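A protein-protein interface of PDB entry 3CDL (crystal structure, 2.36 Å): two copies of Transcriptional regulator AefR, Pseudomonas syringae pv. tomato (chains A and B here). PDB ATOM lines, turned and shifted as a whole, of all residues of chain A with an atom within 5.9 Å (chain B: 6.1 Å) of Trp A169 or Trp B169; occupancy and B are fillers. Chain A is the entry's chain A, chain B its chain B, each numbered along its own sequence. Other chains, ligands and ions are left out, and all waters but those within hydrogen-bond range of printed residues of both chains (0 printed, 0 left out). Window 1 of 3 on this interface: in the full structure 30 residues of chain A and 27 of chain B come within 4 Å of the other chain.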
ATOM      1  N   VAL A 110     -24.089  23.079  -3.894  1.00  0.00           N
ATOM      2  CA  VAL A 110     -22.961  23.957  -3.594  1.00  0.00           C
ATOM      3  C   VAL A 110     -23.096  25.272  -4.373  1.00  0.00           C
ATOM      4  O   VAL A 110     -22.887  26.359  -3.814  1.00  0.00           O
ATOM      5  CB  VAL A 110     -21.554  23.313  -3.871  1.00  0.00           C
ATOM      6  CG1 VAL A 110     -20.447  24.304  -3.532  1.00  0.00           C
ATOM      7  CG2 VAL A 110     -21.327  22.020  -3.067  1.00  0.00           C
ATOM      8  N   LYS A 164     -12.800  14.579   1.031  1.00  0.00           N
ATOM      9  CA  LYS A 164     -13.448  15.633   0.241  1.00  0.00           C
ATOM     10  C   LYS A 164     -12.461  16.459  -0.543  1.00  0.00           C
ATOM     11  O   LYS A 164     -12.774  16.870  -1.669  1.00  0.00           O
ATOM     12  CB  LYS A 164     -14.257  16.567   1.145  1.00  0.00           C
ATOM     13  CG  LYS A 164     -15.624  16.019   1.513  1.00  0.00           C
ATOM     14  CD  LYS A 164     -16.374  16.930   2.480  1.00  0.00           C
ATOM     15  CE  LYS A 164     -17.117  18.044   1.752  1.00  0.00           C
ATOM     16  NZ  LYS A 164     -17.931  18.884   2.681  1.00  0.00           N
ATOM     17  N   SER A 165     -11.283  16.705   0.045  1.00  0.00           N
ATOM     18  CA  SER A 165     -10.223  17.473  -0.637  1.00  0.00           C
ATOM     19  C   SER A 165      -9.740  16.854  -1.942  1.00  0.00           C
ATOM     20  O   SER A 165      -9.165  17.551  -2.782  1.00  0.00           O
ATOM     21  CB  SER A 165      -9.008  17.733   0.277  1.00  0.00           C
ATOM     22  OG  SER A 165      -8.506  16.553   0.884  1.00  0.00           O
ATOM     23  N   PHE A 166      -9.966  15.560  -2.111  1.00  0.00           N
ATOM     24  CA  PHE A 166      -9.417  14.821  -3.243  1.00  0.00           C
ATOM     25  C   PHE A 166     -10.524  14.465  -4.216  1.00  0.00           C
ATOM     26  O   PHE A 166     -10.293  14.346  -5.427  1.00  0.00           O
ATOM     27  CB  PHE A 166      -8.798  13.510  -2.764  1.00  0.00           C
ATOM     28  CG  PHE A 166      -7.479  13.666  -2.039  1.00  0.00           C
ATOM     29  CD1 PHE A 166      -6.275  13.818  -2.757  1.00  0.00           C
ATOM     30  CD2 PHE A 166      -7.419  13.606  -0.632  1.00  0.00           C
ATOM     31  CE1 PHE A 166      -5.067  13.950  -2.086  1.00  0.00           C
ATOM     32  CE2 PHE A 166      -6.208  13.722   0.027  1.00  0.00           C
ATOM     33  CZ  PHE A 166      -5.018  13.885  -0.709  1.00  0.00           C
ATOM     34  N   ALA A 167     -11.722  14.274  -3.667  1.00  0.00           N
ATOM     35  CA  ALA A 167     -12.772  13.519  -4.328  1.00  0.00           C
ATOM     36  C   ALA A 167     -14.134  14.197  -4.219  1.00  0.00           C
ATOM     37  O   ALA A 167     -15.158  13.634  -4.638  1.00  0.00           O
ATOM     38  CB  ALA A 167     -12.835  12.137  -3.736  1.00  0.00           C
ATOM     39  N   PHE A 168     -14.147  15.401  -3.633  1.00  0.00           N
ATOM     40  CA  PHE A 168     -15.327  16.214  -3.650  1.00  0.00           C
ATOM     41  C   PHE A 168     -15.076  17.643  -4.220  1.00  0.00           C
ATOM     42  O   PHE A 168     -15.570  17.975  -5.309  1.00  0.00           O
ATOM     43  CB  PHE A 168     -15.975  16.219  -2.272  1.00  0.00           C
ATOM     44  CG  PHE A 168     -17.226  17.012  -2.202  1.00  0.00           C
ATOM     45  CD1 PHE A 168     -18.436  16.441  -2.545  1.00  0.00           C
ATOM     46  CD2 PHE A 168     -17.197  18.315  -1.790  1.00  0.00           C
ATOM     47  CE1 PHE A 168     -19.600  17.191  -2.480  1.00  0.00           C
ATOM     48  CE2 PHE A 168     -18.354  19.071  -1.727  1.00  0.00           C
ATOM     49  CZ  PHE A 168     -19.536  18.528  -2.083  1.00  0.00           C
ATOM     50  N   TRP A 169     -14.325  18.476  -3.511  1.00  0.00           N
ATOM     51  CA  TRP A 169     -14.036  19.832  -3.984  1.00  0.00           C
ATOM     52  C   TRP A 169     -13.515  19.992  -5.442  1.00  0.00           C
ATOM     53  O   TRP A 169     -14.086  20.781  -6.196  1.00  0.00           O
ATOM     54  CB  TRP A 169     -13.137  20.531  -2.983  1.00  0.00           C
ATOM     55  CG  TRP A 169     -13.841  20.693  -1.659  1.00  0.00           C
ATOM     56  CD1 TRP A 169     -13.475  20.151  -0.462  1.00  0.00           C
ATOM     57  CD2 TRP A 169     -15.080  21.390  -1.425  1.00  0.00           C
ATOM     58  NE1 TRP A 169     -14.386  20.495   0.503  1.00  0.00           N
ATOM     59  CE2 TRP A 169     -15.382  21.253  -0.059  1.00  0.00           C
ATOM     60  CE3 TRP A 169     -15.959  22.106  -2.240  1.00  0.00           C
ATOM     61  CZ2 TRP A 169     -16.528  21.834   0.521  1.00  0.00           C
ATOM     62  CZ3 TRP A 169     -17.096  22.677  -1.661  1.00  0.00           C
ATOM     63  CH2 TRP A 169     -17.366  22.541  -0.298  1.00  0.00           C
ATOM     64  N   PRO A 170     -12.436  19.252  -5.844  1.00  0.00           N
ATOM     65  CA  PRO A 170     -11.974  19.403  -7.228  1.00  0.00           C
ATOM     66  C   PRO A 170     -13.050  19.154  -8.292  1.00  0.00           C
ATOM     67  O   PRO A 170     -13.091  19.847  -9.317  1.00  0.00           O
ATOM     68  CB  PRO A 170     -10.861  18.344  -7.339  1.00  0.00           C
ATOM     69  CG  PRO A 170     -10.353  18.218  -5.977  1.00  0.00           C
ATOM     70  CD  PRO A 170     -11.576  18.296  -5.113  1.00  0.00           C
ATOM     71  N   GLN A 171     -13.915  18.188  -8.021  1.00  0.00           N
ATOM     72  CA  GLN A 171     -14.814  17.636  -9.011  1.00  0.00           C
ATOM     73  C   GLN A 171     -16.007  18.556  -9.133  1.00  0.00           C
ATOM     74  O   GLN A 171     -16.557  18.758 -10.214  1.00  0.00           O
ATOM     75  CB  GLN A 171     -15.286  16.270  -8.549  1.00  0.00           C
ATOM     76  CG  GLN A 171     -14.329  15.119  -8.852  1.00  0.00           C
ATOM     77  CD  GLN A 171     -13.170  14.957  -7.875  1.00  0.00           C
ATOM     78  OE1 GLN A 171     -13.158  15.543  -6.785  1.00  0.00           O
ATOM     79  NE2 GLN A 171     -12.172  14.144  -8.276  1.00  0.00           N
ATOM     80  N   VAL A 172     -16.376  19.116  -8.001  1.00  0.00           N
ATOM     81  CA  VAL A 172     -17.542  19.926  -7.851  1.00  0.00           C
ATOM     82  C   VAL A 172     -17.234  21.386  -8.236  1.00  0.00           C
ATOM     83  O   VAL A 172     -18.075  22.059  -8.848  1.00  0.00           O
ATOM     84  CB  VAL A 172     -18.055  19.796  -6.402  1.00  0.00           C
ATOM     85  CG1 VAL A 172     -19.035  20.920  -6.030  1.00  0.00           C
ATOM     86  CG2 VAL A 172     -18.703  18.435  -6.202  1.00  0.00           C
ATOM     87  N   THR A 173     -16.034  21.875  -7.917  1.00  0.00           N
ATOM     88  CA  THR A 173     -15.715  23.272  -8.247  1.00  0.00           C
ATOM     89  C   THR A 173     -15.093  23.470  -9.627  1.00  0.00           C
ATOM     90  O   THR A 173     -15.242  24.552 -10.182  1.00  0.00           O
ATOM     91  CB  THR A 173     -14.878  23.991  -7.150  1.00  0.00           C
ATOM     92  OG1 THR A 173     -13.565  23.440  -7.121  1.00  0.00           O
ATOM     93  CG2 THR A 173     -15.533  23.845  -5.762  1.00  0.00           C
ATOM     94  N   PHE A 174     -14.392  22.453 -10.165  1.00  0.00           N
ATOM     95  CA  PHE A 174     -13.846  22.522 -11.539  1.00  0.00           C
ATOM     96  C   PHE A 174     -13.855  21.189 -12.336  1.00  0.00           C
ATOM     97  O   PHE A 174     -12.967  20.913 -13.131  1.00  0.00           O
ATOM     98  CB  PHE A 174     -12.456  23.214 -11.585  1.00  0.00           C
ATOM     99  CG  PHE A 174     -11.436  22.606 -10.672  1.00  0.00           C
ATOM    100  CD1 PHE A 174     -11.316  23.050  -9.345  1.00  0.00           C
ATOM    101  CD2 PHE A 174     -10.583  21.595 -11.128  1.00  0.00           C
ATOM    102  CE1 PHE A 174     -10.373  22.478  -8.469  1.00  0.00           C
ATOM    103  CE2 PHE A 174      -9.632  21.013 -10.264  1.00  0.00           C
ATOM    104  CZ  PHE A 174      -9.522  21.466  -8.934  1.00  0.00           C
ATOM    105  N   VAL B 110     -14.779  30.687  -7.562  1.00  0.00           N
ATOM    106  CA  VAL B 110     -15.522  29.453  -7.432  1.00  0.00           C
ATOM    107  C   VAL B 110     -16.916  29.565  -8.037  1.00  0.00           C
ATOM    108  O   VAL B 110     -17.360  28.677  -8.770  1.00  0.00           O
ATOM    109  CB  VAL B 110     -15.627  29.021  -5.959  1.00  0.00           C
ATOM    110  CG1 VAL B 110     -16.459  27.722  -5.843  1.00  0.00           C
ATOM    111  CG2 VAL B 110     -14.233  28.834  -5.381  1.00  0.00           C
ATOM    112  N   LYS B 164      -8.482  24.289   5.371  1.00  0.00           N
ATOM    113  CA  LYS B 164      -9.509  24.785   4.479  1.00  0.00           C
ATOM    114  C   LYS B 164     -10.880  24.305   4.912  1.00  0.00           C
ATOM    115  O   LYS B 164     -11.843  24.976   4.694  1.00  0.00           O
ATOM    116  CB  LYS B 164      -9.210  24.335   3.055  1.00  0.00           C
ATOM    117  CG  LYS B 164      -8.347  25.293   2.203  1.00  0.00           C
ATOM    118  CD  LYS B 164      -7.247  24.557   1.395  1.00  0.00           C
ATOM    119  CE  LYS B 164      -7.346  24.835  -0.098  1.00  0.00           C
ATOM    120  NZ  LYS B 164      -8.611  24.216  -0.592  1.00  0.00           N
ATOM    121  N   SER B 165     -10.955  23.146   5.556  1.00  0.00           N
ATOM    122  CA  SER B 165     -12.249  22.526   5.886  1.00  0.00           C
ATOM    123  C   SER B 165     -12.970  23.306   6.985  1.00  0.00           C
ATOM    124  O   SER B 165     -14.184  23.169   7.159  1.00  0.00           O
ATOM    125  CB  SER B 165     -12.071  21.057   6.278  1.00  0.00           C
ATOM    126  OG  SER B 165     -11.275  20.920   7.450  1.00  0.00           O
ATOM    127  N   PHE B 166     -12.208  24.142   7.683  1.00  0.00           N
ATOM    128  CA  PHE B 166     -12.719  25.042   8.729  1.00  0.00           C
ATOM    129  C   PHE B 166     -12.660  26.509   8.312  1.00  0.00           C
ATOM    130  O   PHE B 166     -13.539  27.301   8.651  1.00  0.00           O
ATOM    131  CB  PHE B 166     -11.907  24.897  10.038  1.00  0.00           C
ATOM    132  CG  PHE B 166     -11.998  23.531  10.657  1.00  0.00           C
ATOM    133  CD1 PHE B 166     -13.176  23.117  11.300  1.00  0.00           C
ATOM    134  CD2 PHE B 166     -10.918  22.638  10.575  1.00  0.00           C
ATOM    135  CE1 PHE B 166     -13.267  21.854  11.869  1.00  0.00           C
ATOM    136  CE2 PHE B 166     -10.999  21.374  11.131  1.00  0.00           C
ATOM    137  CZ  PHE B 166     -12.168  20.979  11.776  1.00  0.00           C
ATOM    138  N   ALA B 167     -11.592  26.879   7.610  1.00  0.00           N
ATOM    139  CA  ALA B 167     -11.314  28.276   7.372  1.00  0.00           C
ATOM    140  C   ALA B 167     -11.475  28.688   5.904  1.00  0.00           C
ATOM    141  O   ALA B 167     -11.183  29.837   5.530  1.00  0.00           O
ATOM    142  CB  ALA B 167      -9.935  28.620   7.897  1.00  0.00           C
ATOM    143  N   PHE B 168     -11.940  27.782   5.054  1.00  0.00           N
ATOM    144  CA  PHE B 168     -12.128  28.182   3.666  1.00  0.00           C
ATOM    145  C   PHE B 168     -13.502  27.808   3.126  1.00  0.00           C
ATOM    146  O   PHE B 168     -14.357  28.693   2.986  1.00  0.00           O
ATOM    147  CB  PHE B 168     -10.986  27.693   2.802  1.00  0.00           C
ATOM    148  CG  PHE B 168     -11.088  28.119   1.377  1.00  0.00           C
ATOM    149  CD1 PHE B 168     -10.737  29.427   0.994  1.00  0.00           C
ATOM    150  CD2 PHE B 168     -11.521  27.214   0.400  1.00  0.00           C
ATOM    151  CE1 PHE B 168     -10.832  29.832  -0.335  1.00  0.00           C
ATOM    152  CE2 PHE B 168     -11.627  27.600  -0.916  1.00  0.00           C
ATOM    153  CZ  PHE B 168     -11.268  28.919  -1.293  1.00  0.00           C
ATOM    154  N   TRP B 169     -13.729  26.523   2.845  1.00  0.00           N
ATOM    155  CA  TRP B 169     -15.036  26.064   2.379  1.00  0.00           C
ATOM    156  C   TRP B 169     -16.284  26.555   3.143  1.00  0.00           C
ATOM    157  O   TRP B 169     -17.201  27.043   2.511  1.00  0.00           O
ATOM    158  CB  TRP B 169     -15.045  24.551   2.214  1.00  0.00           C
ATOM    159  CG  TRP B 169     -14.023  24.116   1.189  1.00  0.00           C
ATOM    160  CD1 TRP B 169     -12.915  23.340   1.405  1.00  0.00           C
ATOM    161  CD2 TRP B 169     -14.019  24.443  -0.201  1.00  0.00           C
ATOM    162  NE1 TRP B 169     -12.215  23.151   0.218  1.00  0.00           N
ATOM    163  CE2 TRP B 169     -12.870  23.824  -0.780  1.00  0.00           C
ATOM    164  CE3 TRP B 169     -14.856  25.215  -1.018  1.00  0.00           C
ATOM    165  CZ2 TRP B 169     -12.557  23.939  -2.148  1.00  0.00           C
ATOM    166  CZ3 TRP B 169     -14.540  25.336  -2.387  1.00  0.00           C
ATOM    167  CH2 TRP B 169     -13.408  24.694  -2.932  1.00  0.00           C
ATOM    168  N   PRO B 170     -16.354  26.409   4.488  1.00  0.00           N
ATOM    169  CA  PRO B 170     -17.529  27.007   5.135  1.00  0.00           C
ATOM    170  C   PRO B 170     -17.780  28.461   4.764  1.00  0.00           C
ATOM    171  O   PRO B 170     -18.929  28.865   4.593  1.00  0.00           O
ATOM    172  CB  PRO B 170     -17.210  26.864   6.630  1.00  0.00           C
ATOM    173  CG  PRO B 170     -16.463  25.572   6.691  1.00  0.00           C
ATOM    174  CD  PRO B 170     -15.525  25.681   5.476  1.00  0.00           C
ATOM    175  N   GLN B 171     -16.711  29.233   4.619  1.00  0.00           N
ATOM    176  CA  GLN B 171     -16.851  30.653   4.374  1.00  0.00           C
ATOM    177  C   GLN B 171     -17.252  30.936   2.914  1.00  0.00           C
ATOM    178  O   GLN B 171     -18.064  31.837   2.629  1.00  0.00           O
ATOM    179  CB  GLN B 171     -15.556  31.390   4.744  1.00  0.00           C
ATOM    180  CG  GLN B 171     -15.290  31.470   6.238  1.00  0.00           C
ATOM    181  CD  GLN B 171     -14.746  30.162   6.827  1.00  0.00           C
ATOM    182  OE1 GLN B 171     -14.335  29.279   6.100  1.00  0.00           O
ATOM    183  NE2 GLN B 171     -14.760  30.048   8.153  1.00  0.00           N
ATOM    184  N   VAL B 172     -16.684  30.143   2.008  1.00  0.00           N
ATOM    185  CA  VAL B 172     -16.896  30.310   0.584  1.00  0.00           C
ATOM    186  C   VAL B 172     -18.271  29.765   0.226  1.00  0.00           C
ATOM    187  O   VAL B 172     -18.968  30.326  -0.604  1.00  0.00           O
ATOM    188  CB  VAL B 172     -15.757  29.613  -0.254  1.00  0.00           C
ATOM    189  CG1 VAL B 172     -16.213  29.270  -1.667  1.00  0.00           C
ATOM    190  CG2 VAL B 172     -14.504  30.458  -0.288  1.00  0.00           C
ATOM    191  N   THR B 173     -18.689  28.683   0.857  1.00  0.00           N
ATOM    192  CA  THR B 173     -19.915  28.014   0.415  1.00  0.00           C
ATOM    193  C   THR B 173     -21.146  28.456   1.194  1.00  0.00           C
ATOM    194  O   THR B 173     -22.228  28.554   0.631  1.00  0.00           O
ATOM    195  CB  THR B 173     -19.771  26.456   0.377  1.00  0.00           C
ATOM    196  OG1 THR B 173     -19.501  25.970   1.695  1.00  0.00           O
ATOM    197  CG2 THR B 173     -18.607  26.060  -0.486  1.00  0.00           C
ATOM    198  N   PHE B 174     -20.981  28.739   2.478  1.00  0.00           N
ATOM    199  CA  PHE B 174     -22.132  29.038   3.340  1.00  0.00           C
ATOM    200  C   PHE B 174     -22.091  30.441   3.924  1.00  0.00           C
ATOM    201  O   PHE B 174     -22.915  30.785   4.768  1.00  0.00           O
ATOM    202  CB  PHE B 174     -22.223  28.010   4.486  1.00  0.00           C
ATOM    203  CG  PHE B 174     -22.513  26.602   4.027  1.00  0.00           C
ATOM    204  CD1 PHE B 174     -23.735  26.284   3.418  1.00  0.00           C
ATOM    205  CD2 PHE B 174     -21.571  25.580   4.211  1.00  0.00           C
ATOM    206  CE1 PHE B 174     -24.009  24.977   2.987  1.00  0.00           C
ATOM    207  CE2 PHE B 174     -21.841  24.267   3.774  1.00  0.00           C
ATOM    208  CZ  PHE B 174     -23.064  23.975   3.164  1.00  0.00           C
ATOM    209  N   ASN B 175     -21.145  31.253   3.467  1.00  0.00           N
ATOM    210  CA  ASN B 175     -20.781  32.502   4.163  1.00  0.00           C
ATOM    211  C   ASN B 175     -20.747  32.300   5.665  1.00  0.00           C
ATOM    212  O   ASN B 175     -21.502  32.923   6.410  1.00  0.00           O
ATOM    213  CB  ASN B 175     -21.689  33.671   3.778  1.00  0.00           C
ATOM    214  CG  ASN B 175     -21.037  34.612   2.771  1.00  0.00           C
ATOM    215  OD1 ASN B 175     -21.246  34.490   1.560  1.00  0.00           O
ATOM    216  ND2 ASN B 175     -20.234  35.551   3.270  1.00  0.00           N
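NE1 of Trp A169 lies close to NE1 of Trp B169.
The backbone carbonyl oxygen of Lys A164 is in hydrogen-bond range of the backbone NH of Trp A169 (2.9 Å). The backbone carbonyl oxygen (O) of Trp A169 sits at hydrogen-bond distance from the side-chain hydroxyl (OG1) of Thr A173, at 2.9 Å. N of Trp B169 lies within hydrogen-bond range of O of Lys B164. The backbone carbonyl oxygen (O) of Trp B169 lies within hydrogen-bond range of the side-chain hydroxyl (OG1) of Thr B173 (2.7 Å).
Among the printed residues, merely in contact across the chains: Thr A173 with Trp B169 (3.6 Å), Trp A169 with Thr B173 (3.7 Å), Val A110 with Thr B173 (3.97 Å) and Thr A173 with Val B110 (3.99 Å).
Of the printed residues of chain B, Val A110 touches Thr B173. Of chain B, only Trp B169 and Thr B173 come within 4 Å of Trp A169. Of the printed residues of chain A, Val B110 touches Thr A173. Trp B169 touches just these residues of chain A: Trp A169 (3.3 Å) and Thr A173 (3.6 Å). The nearest printed residue of chain B that does not touch Val A110 is Val B110 (5.7 Å).
Printed residues of chain B that touch a printed residue of chain A: Val B110, Trp B169 and Thr B173. Hydrophobic or aromatic side chains of chain B within 4 Å of the printed part of chain A: Val B110 and Trp B169. Of the 12 printed residues of chain A, 3 touch a printed residue of chain B. Hydrophobic or aromatic side chains of chain A within 4 Å of the printed part of chain B: Val A110 and Trp A169. Among the printed residues, 5 pairs touch across the chains. Among the printed residues, no Asp or Glu carboxylate lies within 4 Å of a Lys or Arg side-chain nitrogen of the other chain.
Val A110 touches Thr B173, and with the chains exchanged Thr A173 touches Val B110. Trp A169 touches its own counterpart, Trp B169. Trp A169 touches Thr B173, and with the chains exchanged Thr A173 touches Trp B169. Of the 5 pairs that touch across the chains among the printed residues, 5 have their exchanged pair printed and touching as well.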
